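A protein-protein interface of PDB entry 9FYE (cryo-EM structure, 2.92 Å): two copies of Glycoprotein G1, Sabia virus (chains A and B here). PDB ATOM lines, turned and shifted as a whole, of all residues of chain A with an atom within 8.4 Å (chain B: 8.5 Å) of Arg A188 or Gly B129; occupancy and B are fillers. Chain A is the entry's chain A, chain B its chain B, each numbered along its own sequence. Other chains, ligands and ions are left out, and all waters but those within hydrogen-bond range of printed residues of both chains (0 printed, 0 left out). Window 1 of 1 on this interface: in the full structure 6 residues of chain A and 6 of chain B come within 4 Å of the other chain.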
ATOM      1  N   HIS A  23      44.326 -13.654  24.434  1.00  0.00           N
ATOM      2  CA  HIS A  23      43.131 -14.450  24.649  1.00  0.00           C
ATOM      3  C   HIS A  23      43.090 -14.975  26.076  1.00  0.00           C
ATOM      4  O   HIS A  23      44.138 -15.159  26.700  1.00  0.00           O
ATOM      5  CB  HIS A  23      43.084 -15.622  23.662  1.00  0.00           C
ATOM      6  CG  HIS A  23      42.979 -15.199  22.231  1.00  0.00           C
ATOM      7  ND1 HIS A  23      44.040 -15.269  21.356  1.00  0.00           N
ATOM      8  CD2 HIS A  23      41.939 -14.704  21.522  1.00  0.00           C
ATOM      9  CE1 HIS A  23      43.660 -14.830  20.170  1.00  0.00           C
ATOM     10  NE2 HIS A  23      42.389 -14.483  20.244  1.00  0.00           N
ATOM     11  N   PRO A  24      41.892 -15.201  26.623  1.00  0.00           N
ATOM     12  CA  PRO A  24      41.788 -15.598  28.033  1.00  0.00           C
ATOM     13  C   PRO A  24      42.542 -16.886  28.320  1.00  0.00           C
ATOM     14  O   PRO A  24      42.462 -17.859  27.568  1.00  0.00           O
ATOM     15  CB  PRO A  24      40.280 -15.768  28.243  1.00  0.00           C
ATOM     16  CG  PRO A  24      39.658 -14.922  27.197  1.00  0.00           C
ATOM     17  CD  PRO A  24      40.569 -14.986  26.014  1.00  0.00           C
ATOM     18  N   GLY A  84      32.280 -10.383  31.383  1.00  0.00           N
ATOM     19  CA  GLY A  84      32.520 -11.315  30.297  1.00  0.00           C
ATOM     20  C   GLY A  84      33.407 -12.466  30.722  1.00  0.00           C
ATOM     21  O   GLY A  84      33.126 -13.625  30.419  1.00  0.00           O
ATOM     22  N   GLU A  87      31.465 -14.835  32.854  1.00  0.00           N
ATOM     23  CA  GLU A  87      30.627 -15.696  32.029  1.00  0.00           C
ATOM     24  C   GLU A  87      31.452 -16.779  31.345  1.00  0.00           C
ATOM     25  O   GLU A  87      30.992 -17.913  31.193  1.00  0.00           O
ATOM     26  CB  GLU A  87      29.880 -14.851  31.002  1.00  0.00           C
ATOM     27  CG  GLU A  87      28.826 -13.954  31.614  1.00  0.00           C
ATOM     28  CD  GLU A  87      28.234 -12.994  30.610  1.00  0.00           C
ATOM     29  OE1 GLU A  87      28.706 -12.987  29.455  1.00  0.00           O
ATOM     30  OE2 GLU A  87      27.299 -12.251  30.973  1.00  0.00           O
ATOM     31  N   TRP A  88      32.673 -16.442  30.927  1.00  0.00           N
ATOM     32  CA  TRP A  88      33.609 -17.446  30.422  1.00  0.00           C
ATOM     33  C   TRP A  88      33.881 -18.535  31.450  1.00  0.00           C
ATOM     34  O   TRP A  88      33.872 -19.726  31.121  1.00  0.00           O
ATOM     35  CB  TRP A  88      34.912 -16.765  29.996  1.00  0.00           C
ATOM     36  CG  TRP A  88      34.903 -16.215  28.607  1.00  0.00           C
ATOM     37  CD1 TRP A  88      34.272 -15.096  28.166  1.00  0.00           C
ATOM     38  CD2 TRP A  88      35.691 -16.688  27.508  1.00  0.00           C
ATOM     39  NE1 TRP A  88      34.541 -14.894  26.834  1.00  0.00           N
ATOM     40  CE2 TRP A  88      35.422 -15.852  26.412  1.00  0.00           C
ATOM     41  CE3 TRP A  88      36.576 -17.756  27.340  1.00  0.00           C
ATOM     42  CZ2 TRP A  88      36.004 -16.050  25.164  1.00  0.00           C
ATOM     43  CZ3 TRP A  88      37.148 -17.952  26.102  1.00  0.00           C
ATOM     44  CH2 TRP A  88      36.862 -17.105  25.030  1.00  0.00           C
ATOM     45  N   ARG A  91      30.557 -20.637  31.985  1.00  0.00           N
ATOM     46  CA  ARG A  91      30.307 -21.491  30.831  1.00  0.00           C
ATOM     47  C   ARG A  91      31.327 -22.615  30.745  1.00  0.00           C
ATOM     48  O   ARG A  91      30.997 -23.733  30.334  1.00  0.00           O
ATOM     49  CB  ARG A  91      30.335 -20.651  29.561  1.00  0.00           C
ATOM     50  CG  ARG A  91      29.855 -21.365  28.330  1.00  0.00           C
ATOM     51  CD  ARG A  91      29.721 -20.393  27.185  1.00  0.00           C
ATOM     52  NE  ARG A  91      28.986 -19.194  27.570  1.00  0.00           N
ATOM     53  CZ  ARG A  91      29.497 -17.970  27.578  1.00  0.00           C
ATOM     54  NH1 ARG A  91      30.746 -17.741  27.215  1.00  0.00           N
ATOM     55  NH2 ARG A  91      28.731 -16.949  27.951  1.00  0.00           N
ATOM     56  N   ALA A  92      32.581 -22.330  31.105  1.00  0.00           N
ATOM     57  CA  ALA A  92      33.607 -23.363  31.103  1.00  0.00           C
ATOM     58  C   ALA A  92      33.304 -24.444  32.126  1.00  0.00           C
ATOM     59  O   ALA A  92      33.657 -25.611  31.921  1.00  0.00           O
ATOM     60  CB  ALA A  92      34.974 -22.738  31.363  1.00  0.00           C
ATOM     61  N   MET A 182      39.034 -21.646  25.900  1.00  0.00           N
ATOM     62  CA  MET A 182      38.491 -21.210  24.617  1.00  0.00           C
ATOM     63  C   MET A 182      37.514 -22.222  24.038  1.00  0.00           C
ATOM     64  O   MET A 182      36.492 -21.837  23.465  1.00  0.00           O
ATOM     65  CB  MET A 182      39.608 -20.959  23.615  1.00  0.00           C
ATOM     66  CG  MET A 182      40.214 -19.591  23.689  1.00  0.00           C
ATOM     67  SD  MET A 182      41.493 -19.442  22.448  1.00  0.00           S
ATOM     68  CE  MET A 182      42.850 -18.998  23.500  1.00  0.00           C
ATOM     69  N   LEU A 183      37.818 -23.515  24.139  1.00  0.00           N
ATOM     70  CA  LEU A 183      36.901 -24.514  23.605  1.00  0.00           C
ATOM     71  C   LEU A 183      35.572 -24.474  24.340  1.00  0.00           C
ATOM     72  O   LEU A 183      34.512 -24.649  23.730  1.00  0.00           O
ATOM     73  CB  LEU A 183      37.519 -25.907  23.677  1.00  0.00           C
ATOM     74  CG  LEU A 183      38.409 -26.255  22.486  1.00  0.00           C
ATOM     75  CD1 LEU A 183      39.019 -27.623  22.665  1.00  0.00           C
ATOM     76  CD2 LEU A 183      37.620 -26.186  21.195  1.00  0.00           C
ATOM     77  N   ALA A 184      35.607 -24.255  25.655  1.00  0.00           N
ATOM     78  CA  ALA A 184      34.357 -24.160  26.401  1.00  0.00           C
ATOM     79  C   ALA A 184      33.515 -22.979  25.927  1.00  0.00           C
ATOM     80  O   ALA A 184      32.293 -23.098  25.778  1.00  0.00           O
ATOM     81  CB  ALA A 184      34.651 -24.051  27.892  1.00  0.00           C
ATOM     82  N   ASN A 185      34.144 -21.831  25.691  1.00  0.00           N
ATOM     83  CA  ASN A 185      33.477 -20.634  25.176  1.00  0.00           C
ATOM     84  C   ASN A 185      33.868 -20.447  23.713  1.00  0.00           C
ATOM     85  O   ASN A 185      34.861 -19.790  23.404  1.00  0.00           O
ATOM     86  CB  ASN A 185      33.850 -19.410  25.990  1.00  0.00           C
ATOM     87  CG  ASN A 185      33.658 -19.616  27.466  1.00  0.00           C
ATOM     88  OD1 ASN A 185      32.635 -19.235  28.020  1.00  0.00           O
ATOM     89  ND2 ASN A 185      34.647 -20.211  28.117  1.00  0.00           N
ATOM     90  N   ALA A 186      33.050 -20.974  22.810  1.00  0.00           N
ATOM     91  CA  ALA A 186      33.353 -20.976  21.387  1.00  0.00           C
ATOM     92  C   ALA A 186      32.367 -20.075  20.661  1.00  0.00           C
ATOM     93  O   ALA A 186      31.152 -20.227  20.815  1.00  0.00           O
ATOM     94  CB  ALA A 186      33.303 -22.394  20.817  1.00  0.00           C
ATOM     95  N   GLY A 187      32.892 -19.154  19.858  1.00  0.00           N
ATOM     96  CA  GLY A 187      32.046 -18.199  19.172  1.00  0.00           C
ATOM     97  C   GLY A 187      31.496 -17.101  20.054  1.00  0.00           C
ATOM     98  O   GLY A 187      30.380 -16.629  19.817  1.00  0.00           O
ATOM     99  N   ARG A 188      32.249 -16.679  21.070  1.00  0.00           N
ATOM    100  CA  ARG A 188      31.836 -15.589  21.941  1.00  0.00           C
ATOM    101  C   ARG A 188      33.011 -14.681  22.265  1.00  0.00           C
ATOM    102  O   ARG A 188      34.178 -15.059  22.144  1.00  0.00           O
ATOM    103  CB  ARG A 188      31.227 -16.069  23.266  1.00  0.00           C
ATOM    104  CG  ARG A 188      29.857 -16.672  23.150  1.00  0.00           C
ATOM    105  CD  ARG A 188      29.857 -18.130  22.801  1.00  0.00           C
ATOM    106  NE  ARG A 188      28.478 -18.568  22.649  1.00  0.00           N
ATOM    107  CZ  ARG A 188      27.706 -18.949  23.652  1.00  0.00           C
ATOM    108  NH1 ARG A 188      28.142 -18.949  24.895  1.00  0.00           N
ATOM    109  NH2 ARG A 188      26.452 -19.301  23.407  1.00  0.00           N
ATOM    110  N   SER A 189      32.669 -13.464  22.676  1.00  0.00           N
ATOM    111  CA  SER A 189      33.626 -12.454  23.091  1.00  0.00           C
ATOM    112  C   SER A 189      33.207 -11.926  24.455  1.00  0.00           C
ATOM    113  O   SER A 189      32.065 -12.107  24.885  1.00  0.00           O
ATOM    114  CB  SER A 189      33.713 -11.307  22.078  1.00  0.00           C
ATOM    115  OG  SER A 189      34.088 -11.785  20.799  1.00  0.00           O
ATOM    116  N   SER A 190      34.150 -11.288  25.144  1.00  0.00           N
ATOM    117  CA  SER A 190      33.879 -10.787  26.486  1.00  0.00           C
ATOM    118  C   SER A 190      32.761  -9.752  26.457  1.00  0.00           C
ATOM    119  O   SER A 190      32.751  -8.851  25.614  1.00  0.00           O
ATOM    120  CB  SER A 190      35.145 -10.178  27.088  1.00  0.00           C
ATOM    121  OG  SER A 190      35.519  -8.997  26.400  1.00  0.00           O
ATOM    122  N   GLY A 191      31.821  -9.882  27.387  1.00  0.00           N
ATOM    123  CA  GLY A 191      30.690  -8.976  27.464  1.00  0.00           C
ATOM    124  C   GLY A 191      29.684  -9.365  28.528  1.00  0.00           C
ATOM    125  O   GLY A 191      29.159  -8.512  29.242  1.00  0.00           O
ATOM    126  N   ASP B 100      14.319 -21.934  27.071  1.00  0.00           N
ATOM    127  CA  ASP B 100      14.575 -21.002  25.985  1.00  0.00           C
ATOM    128  C   ASP B 100      13.314 -20.189  25.702  1.00  0.00           C
ATOM    129  O   ASP B 100      12.206 -20.640  26.002  1.00  0.00           O
ATOM    130  CB  ASP B 100      15.028 -21.736  24.727  1.00  0.00           C
ATOM    131  CG  ASP B 100      16.387 -22.382  24.891  1.00  0.00           C
ATOM    132  OD1 ASP B 100      17.041 -22.134  25.923  1.00  0.00           O
ATOM    133  OD2 ASP B 100      16.803 -23.135  23.987  1.00  0.00           O
ATOM    134  N   ILE B 121      15.208 -14.120  19.379  1.00  0.00           N
ATOM    135  CA  ILE B 121      16.606 -14.446  19.625  1.00  0.00           C
ATOM    136  C   ILE B 121      17.422 -13.207  19.971  1.00  0.00           C
ATOM    137  O   ILE B 121      18.653 -13.262  19.975  1.00  0.00           O
ATOM    138  CB  ILE B 121      17.227 -15.200  18.439  1.00  0.00           C
ATOM    139  CG1 ILE B 121      17.177 -14.353  17.171  1.00  0.00           C
ATOM    140  CG2 ILE B 121      16.504 -16.514  18.219  1.00  0.00           C
ATOM    141  CD1 ILE B 121      17.694 -15.070  15.947  1.00  0.00           C
ATOM    142  N   THR B 122      16.764 -12.085  20.246  1.00  0.00           N
ATOM    143  CA  THR B 122      17.471 -10.902  20.710  1.00  0.00           C
ATOM    144  C   THR B 122      18.122 -11.185  22.058  1.00  0.00           C
ATOM    145  O   THR B 122      17.601 -11.949  22.875  1.00  0.00           O
ATOM    146  CB  THR B 122      16.509  -9.721  20.826  1.00  0.00           C
ATOM    147  OG1 THR B 122      15.701  -9.649  19.646  1.00  0.00           O
ATOM    148  CG2 THR B 122      17.273  -8.417  20.983  1.00  0.00           C
ATOM    149  N   GLU B 123      19.283 -10.565  22.283  1.00  0.00           N
ATOM    150  CA  GLU B 123      20.053 -10.838  23.491  1.00  0.00           C
ATOM    151  C   GLU B 123      19.272 -10.481  24.750  1.00  0.00           C
ATOM    152  O   GLU B 123      19.352 -11.189  25.761  1.00  0.00           O
ATOM    153  CB  GLU B 123      21.381 -10.081  23.447  1.00  0.00           C
ATOM    154  CG  GLU B 123      22.380 -10.518  24.508  1.00  0.00           C
ATOM    155  CD  GLU B 123      22.733 -11.994  24.423  1.00  0.00           C
ATOM    156  OE1 GLU B 123      22.633 -12.581  23.324  1.00  0.00           O
ATOM    157  OE2 GLU B 123      23.111 -12.571  25.462  1.00  0.00           O
ATOM    158  N   GLY B 124      18.526  -9.376  24.716  1.00  0.00           N
ATOM    159  CA  GLY B 124      17.801  -8.946  25.903  1.00  0.00           C
ATOM    160  C   GLY B 124      16.726  -9.926  26.332  1.00  0.00           C
ATOM    161  O   GLY B 124      16.598 -10.247  27.517  1.00  0.00           O
ATOM    162  N   GLY B 126      16.266 -13.256  25.561  1.00  0.00           N
ATOM    163  CA  GLY B 126      16.767 -14.546  25.980  1.00  0.00           C
ATOM    164  C   GLY B 126      17.841 -14.438  27.041  1.00  0.00           C
ATOM    165  O   GLY B 126      18.399 -13.373  27.302  1.00  0.00           O
ATOM    166  N   SER B 127      18.129 -15.575  27.668  1.00  0.00           N
ATOM    167  CA  SER B 127      19.247 -15.630  28.592  1.00  0.00           C
ATOM    168  C   SER B 127      20.553 -15.435  27.828  1.00  0.00           C
ATOM    169  O   SER B 127      20.633 -15.667  26.619  1.00  0.00           O
ATOM    170  CB  SER B 127      19.262 -16.961  29.344  1.00  0.00           C
ATOM    171  OG  SER B 127      19.376 -18.053  28.448  1.00  0.00           O
ATOM    172  N   HIS B 128      21.578 -14.986  28.547  1.00  0.00           N
ATOM    173  CA  HIS B 128      22.827 -14.607  27.900  1.00  0.00           C
ATOM    174  C   HIS B 128      23.423 -15.783  27.137  1.00  0.00           C
ATOM    175  O   HIS B 128      23.480 -16.907  27.643  1.00  0.00           O
ATOM    176  CB  HIS B 128      23.829 -14.081  28.926  1.00  0.00           C
ATOM    177  CG  HIS B 128      24.872 -13.187  28.333  1.00  0.00           C
ATOM    178  ND1 HIS B 128      26.013 -13.671  27.731  1.00  0.00           N
ATOM    179  CD2 HIS B 128      24.939 -11.838  28.237  1.00  0.00           C
ATOM    180  CE1 HIS B 128      26.740 -12.659  27.291  1.00  0.00           C
ATOM    181  NE2 HIS B 128      26.112 -11.535  27.589  1.00  0.00           N
ATOM    182  N   GLY B 129      23.864 -15.515  25.908  1.00  0.00           N
ATOM    183  CA  GLY B 129      24.459 -16.522  25.061  1.00  0.00           C
ATOM    184  C   GLY B 129      23.496 -17.254  24.153  1.00  0.00           C
ATOM    185  O   GLY B 129      23.949 -18.011  23.285  1.00  0.00           O
ATOM    186  N   PHE B 130      22.184 -17.061  24.321  1.00  0.00           N
ATOM    187  CA  PHE B 130      21.223 -17.800  23.506  1.00  0.00           C
ATOM    188  C   PHE B 130      21.310 -17.399  22.040  1.00  0.00           C
ATOM    189  O   PHE B 130      21.206 -18.255  21.153  1.00  0.00           O
ATOM    190  CB  PHE B 130      19.803 -17.594  24.024  1.00  0.00           C
ATOM    191  CG  PHE B 130      18.759 -18.265  23.182  1.00  0.00           C
ATOM    192  CD1 PHE B 130      18.735 -19.642  23.058  1.00  0.00           C
ATOM    193  CD2 PHE B 130      17.811 -17.521  22.505  1.00  0.00           C
ATOM    194  CE1 PHE B 130      17.784 -20.262  22.281  1.00  0.00           C
ATOM    195  CE2 PHE B 130      16.855 -18.138  21.726  1.00  0.00           C
ATOM    196  CZ  PHE B 130      16.842 -19.510  21.614  1.00  0.00           C
ATOM    197  N   GLU B 131      21.474 -16.102  21.762  1.00  0.00           N
ATOM    198  CA  GLU B 131      21.554 -15.658  20.375  1.00  0.00           C
ATOM    199  C   GLU B 131      22.745 -16.298  19.680  1.00  0.00           C
ATOM    200  O   GLU B 131      22.647 -16.721  18.520  1.00  0.00           O
ATOM    201  CB  GLU B 131      21.640 -14.136  20.306  1.00  0.00           C
ATOM    202  CG  GLU B 131      21.759 -13.595  18.893  1.00  0.00           C
ATOM    203  CD  GLU B 131      21.642 -12.087  18.833  1.00  0.00           C
ATOM    204  OE1 GLU B 131      21.938 -11.427  19.850  1.00  0.00           O
ATOM    205  OE2 GLU B 131      21.250 -11.561  17.770  1.00  0.00           O
ATOM    206  N   ASP B 132      23.871 -16.407  20.387  1.00  0.00           N
ATOM    207  CA  ASP B 132      25.057 -17.013  19.800  1.00  0.00           C
ATOM    208  C   ASP B 132      24.787 -18.476  19.481  1.00  0.00           C
ATOM    209  O   ASP B 132      25.127 -18.958  18.394  1.00  0.00           O
ATOM    210  CB  ASP B 132      26.253 -16.851  20.735  1.00  0.00           C
ATOM    211  CG  ASP B 132      26.627 -15.394  20.947  1.00  0.00           C
ATOM    212  OD1 ASP B 132      25.856 -14.515  20.508  1.00  0.00           O
ATOM    213  OD2 ASP B 132      27.689 -15.125  21.540  1.00  0.00           O
ATOM    214  N   THR B 133      24.184 -19.204  20.429  1.00  0.00           N
ATOM    215  CA  THR B 133      23.950 -20.626  20.212  1.00  0.00           C
ATOM    216  C   THR B 133      23.023 -20.817  19.027  1.00  0.00           C
ATOM    217  O   THR B 133      23.262 -21.670  18.170  1.00  0.00           O
ATOM    218  CB  THR B 133      23.333 -21.287  21.448  1.00  0.00           C
ATOM    219  OG1 THR B 133      22.072 -20.674  21.744  1.00  0.00           O
ATOM    220  CG2 THR B 133      24.238 -21.203  22.643  1.00  0.00           C
ATOM    221  N   ILE B 134      21.944 -20.033  18.971  1.00  0.00           N
ATOM    222  CA  ILE B 134      20.957 -20.209  17.915  1.00  0.00           C
ATOM    223  C   ILE B 134      21.562 -19.877  16.553  1.00  0.00           C
ATOM    224  O   ILE B 134      21.315 -20.580  15.569  1.00  0.00           O
ATOM    225  CB  ILE B 134      19.681 -19.396  18.223  1.00  0.00           C
ATOM    226  CG1 ILE B 134      18.457 -20.061  17.592  1.00  0.00           C
ATOM    227  CG2 ILE B 134      19.792 -17.950  17.775  1.00  0.00           C
ATOM    228  CD1 ILE B 134      18.058 -21.355  18.257  1.00  0.00           C
ATOM    229  N   LEU B 135      22.365 -18.810  16.466  1.00  0.00           N
ATOM    230  CA  LEU B 135      22.966 -18.458  15.182  1.00  0.00           C
ATOM    231  C   LEU B 135      23.988 -19.500  14.743  1.00  0.00           C
ATOM    232  O   LEU B 135      24.058 -19.852  13.557  1.00  0.00           O
ATOM    233  CB  LEU B 135      23.606 -17.074  15.267  1.00  0.00           C
ATOM    234  CG  LEU B 135      22.641 -15.891  15.371  1.00  0.00           C
ATOM    235  CD1 LEU B 135      23.403 -14.590  15.249  1.00  0.00           C
ATOM    236  CD2 LEU B 135      21.552 -15.974  14.320  1.00  0.00           C
ATOM    237  N   GLN B 136      24.788 -20.007  15.684  1.00  0.00           N
ATOM    238  CA  GLN B 136      25.740 -21.061  15.351  1.00  0.00           C
ATOM    239  C   GLN B 136      25.019 -22.328  14.912  1.00  0.00           C
ATOM    240  O   GLN B 136      25.465 -23.014  13.987  1.00  0.00           O
ATOM    241  CB  GLN B 136      26.653 -21.337  16.543  1.00  0.00           C
ATOM    242  CG  GLN B 136      27.641 -20.216  16.831  1.00  0.00           C
ATOM    243  CD  GLN B 136      28.304 -20.347  18.190  1.00  0.00           C
ATOM    244  OE1 GLN B 136      28.480 -21.450  18.705  1.00  0.00           O
ATOM    245  NE2 GLN B 136      28.669 -19.216  18.780  1.00  0.00           N
ATOM    246  N   ARG B 137      23.917 -22.667  15.583  1.00  0.00           N
ATOM    247  CA  ARG B 137      23.112 -23.809  15.161  1.00  0.00           C
ATOM    248  C   ARG B 137      22.526 -23.601  13.772  1.00  0.00           C
ATOM    249  O   ARG B 137      22.432 -24.547  12.990  1.00  0.00           O
ATOM    250  CB  ARG B 137      22.014 -24.103  16.181  1.00  0.00           C
ATOM    251  CG  ARG B 137      22.534 -24.682  17.487  1.00  0.00           C
ATOM    252  CD  ARG B 137      21.658 -24.293  18.656  1.00  0.00           C
ATOM    253  NE  ARG B 137      22.157 -24.813  19.923  1.00  0.00           N
ATOM    254  CZ  ARG B 137      21.547 -24.644  21.087  1.00  0.00           C
ATOM    255  NH1 ARG B 137      20.407 -23.978  21.180  1.00  0.00           N
ATOM    256  NH2 ARG B 137      22.091 -25.161  22.185  1.00  0.00           N
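Of the printed residues of chain B, Glu A87 touches His B128. Of the printed residues of chain B, Ala A186 touches Gln B136 (3.4 Å). Of the printed residues of chain B, Arg A188 touches Gly B129 (2.8 Å), Asp B132 (3.1 Å), Thr B133 (3.0 Å) and Gln B136 (3.9 Å). Thr B122 touches none of the printed residues of chain A. Of the printed residues of chain A, His B128 touches Glu A87. Gly B129 touches just one residue of chain A: Arg A188 (2.8 Å). Of the printed residues of chain A, Asp B132 touches Gly A187 (3.5 Å) and Arg A188 (3.1 Å). Of the printed residues of chain A, Gln B136 touches Ala A186 (3.4 Å), Gly A187 (3.3 Å) and Arg A188 (3.9 Å). The nearest residue of chain B that does not touch Arg A188 is Phe B130 (4.9 Å). The nearest residue of chain A that does not touch Gly B129 is Arg A91 (5.2 Å).
No position is printed for both chains. Of the 8 pairs that touch across the chains among the printed residues, none has its exchanged pair printed and touching as well.
The guanidinium group of Arg A188 lies within salt-bridge range of the side-chain carboxylate of Asp B132 (3.7 Å). O of Gly A187 is in hydrogen-bond range of NE2 of Gln B136 (3.3 Å). The guanidinium group of Arg A188 sits at hydrogen-bond distance from the backbone carbonyl oxygen of Gly B129. NE2 of Gln B136 is in hydrogen-bond range of O of Ala A186. OE1 of Glu A87 sits close to ND1 of His B128 (3.3 Å).
The backbone NH (N) of Gly B129 lies within hydrogen-bond range of the side-chain carboxylate (OE2) of Glu B123 (3.1 Å). The backbone carbonyl oxygen of Phe B130 is in hydrogen-bond range of the side-chain hydroxyl of Thr B133 (2.6 Å).
Of the 17 printed residues of chain A, 4 touch a printed residue of chain B. Hydrophobic or aromatic side chains of chain B within 4 Å of the printed part of chain A: His B128. Among the printed residues, 8 pairs touch across the chains. Among the printed residues, Asp or Glu carboxylates within 4 Å of a Lys or Arg side-chain nitrogen of the other chain: Arg A188 with Asp B132 (3.7 Å).
Among the printed residues, pairs that only touch across the chains: Gly A187 with Asp B132 (3.5 Å), Arg A188 with Thr B133 (3.0 Å) and Arg A188 with Gln B136 (3.9 Å).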
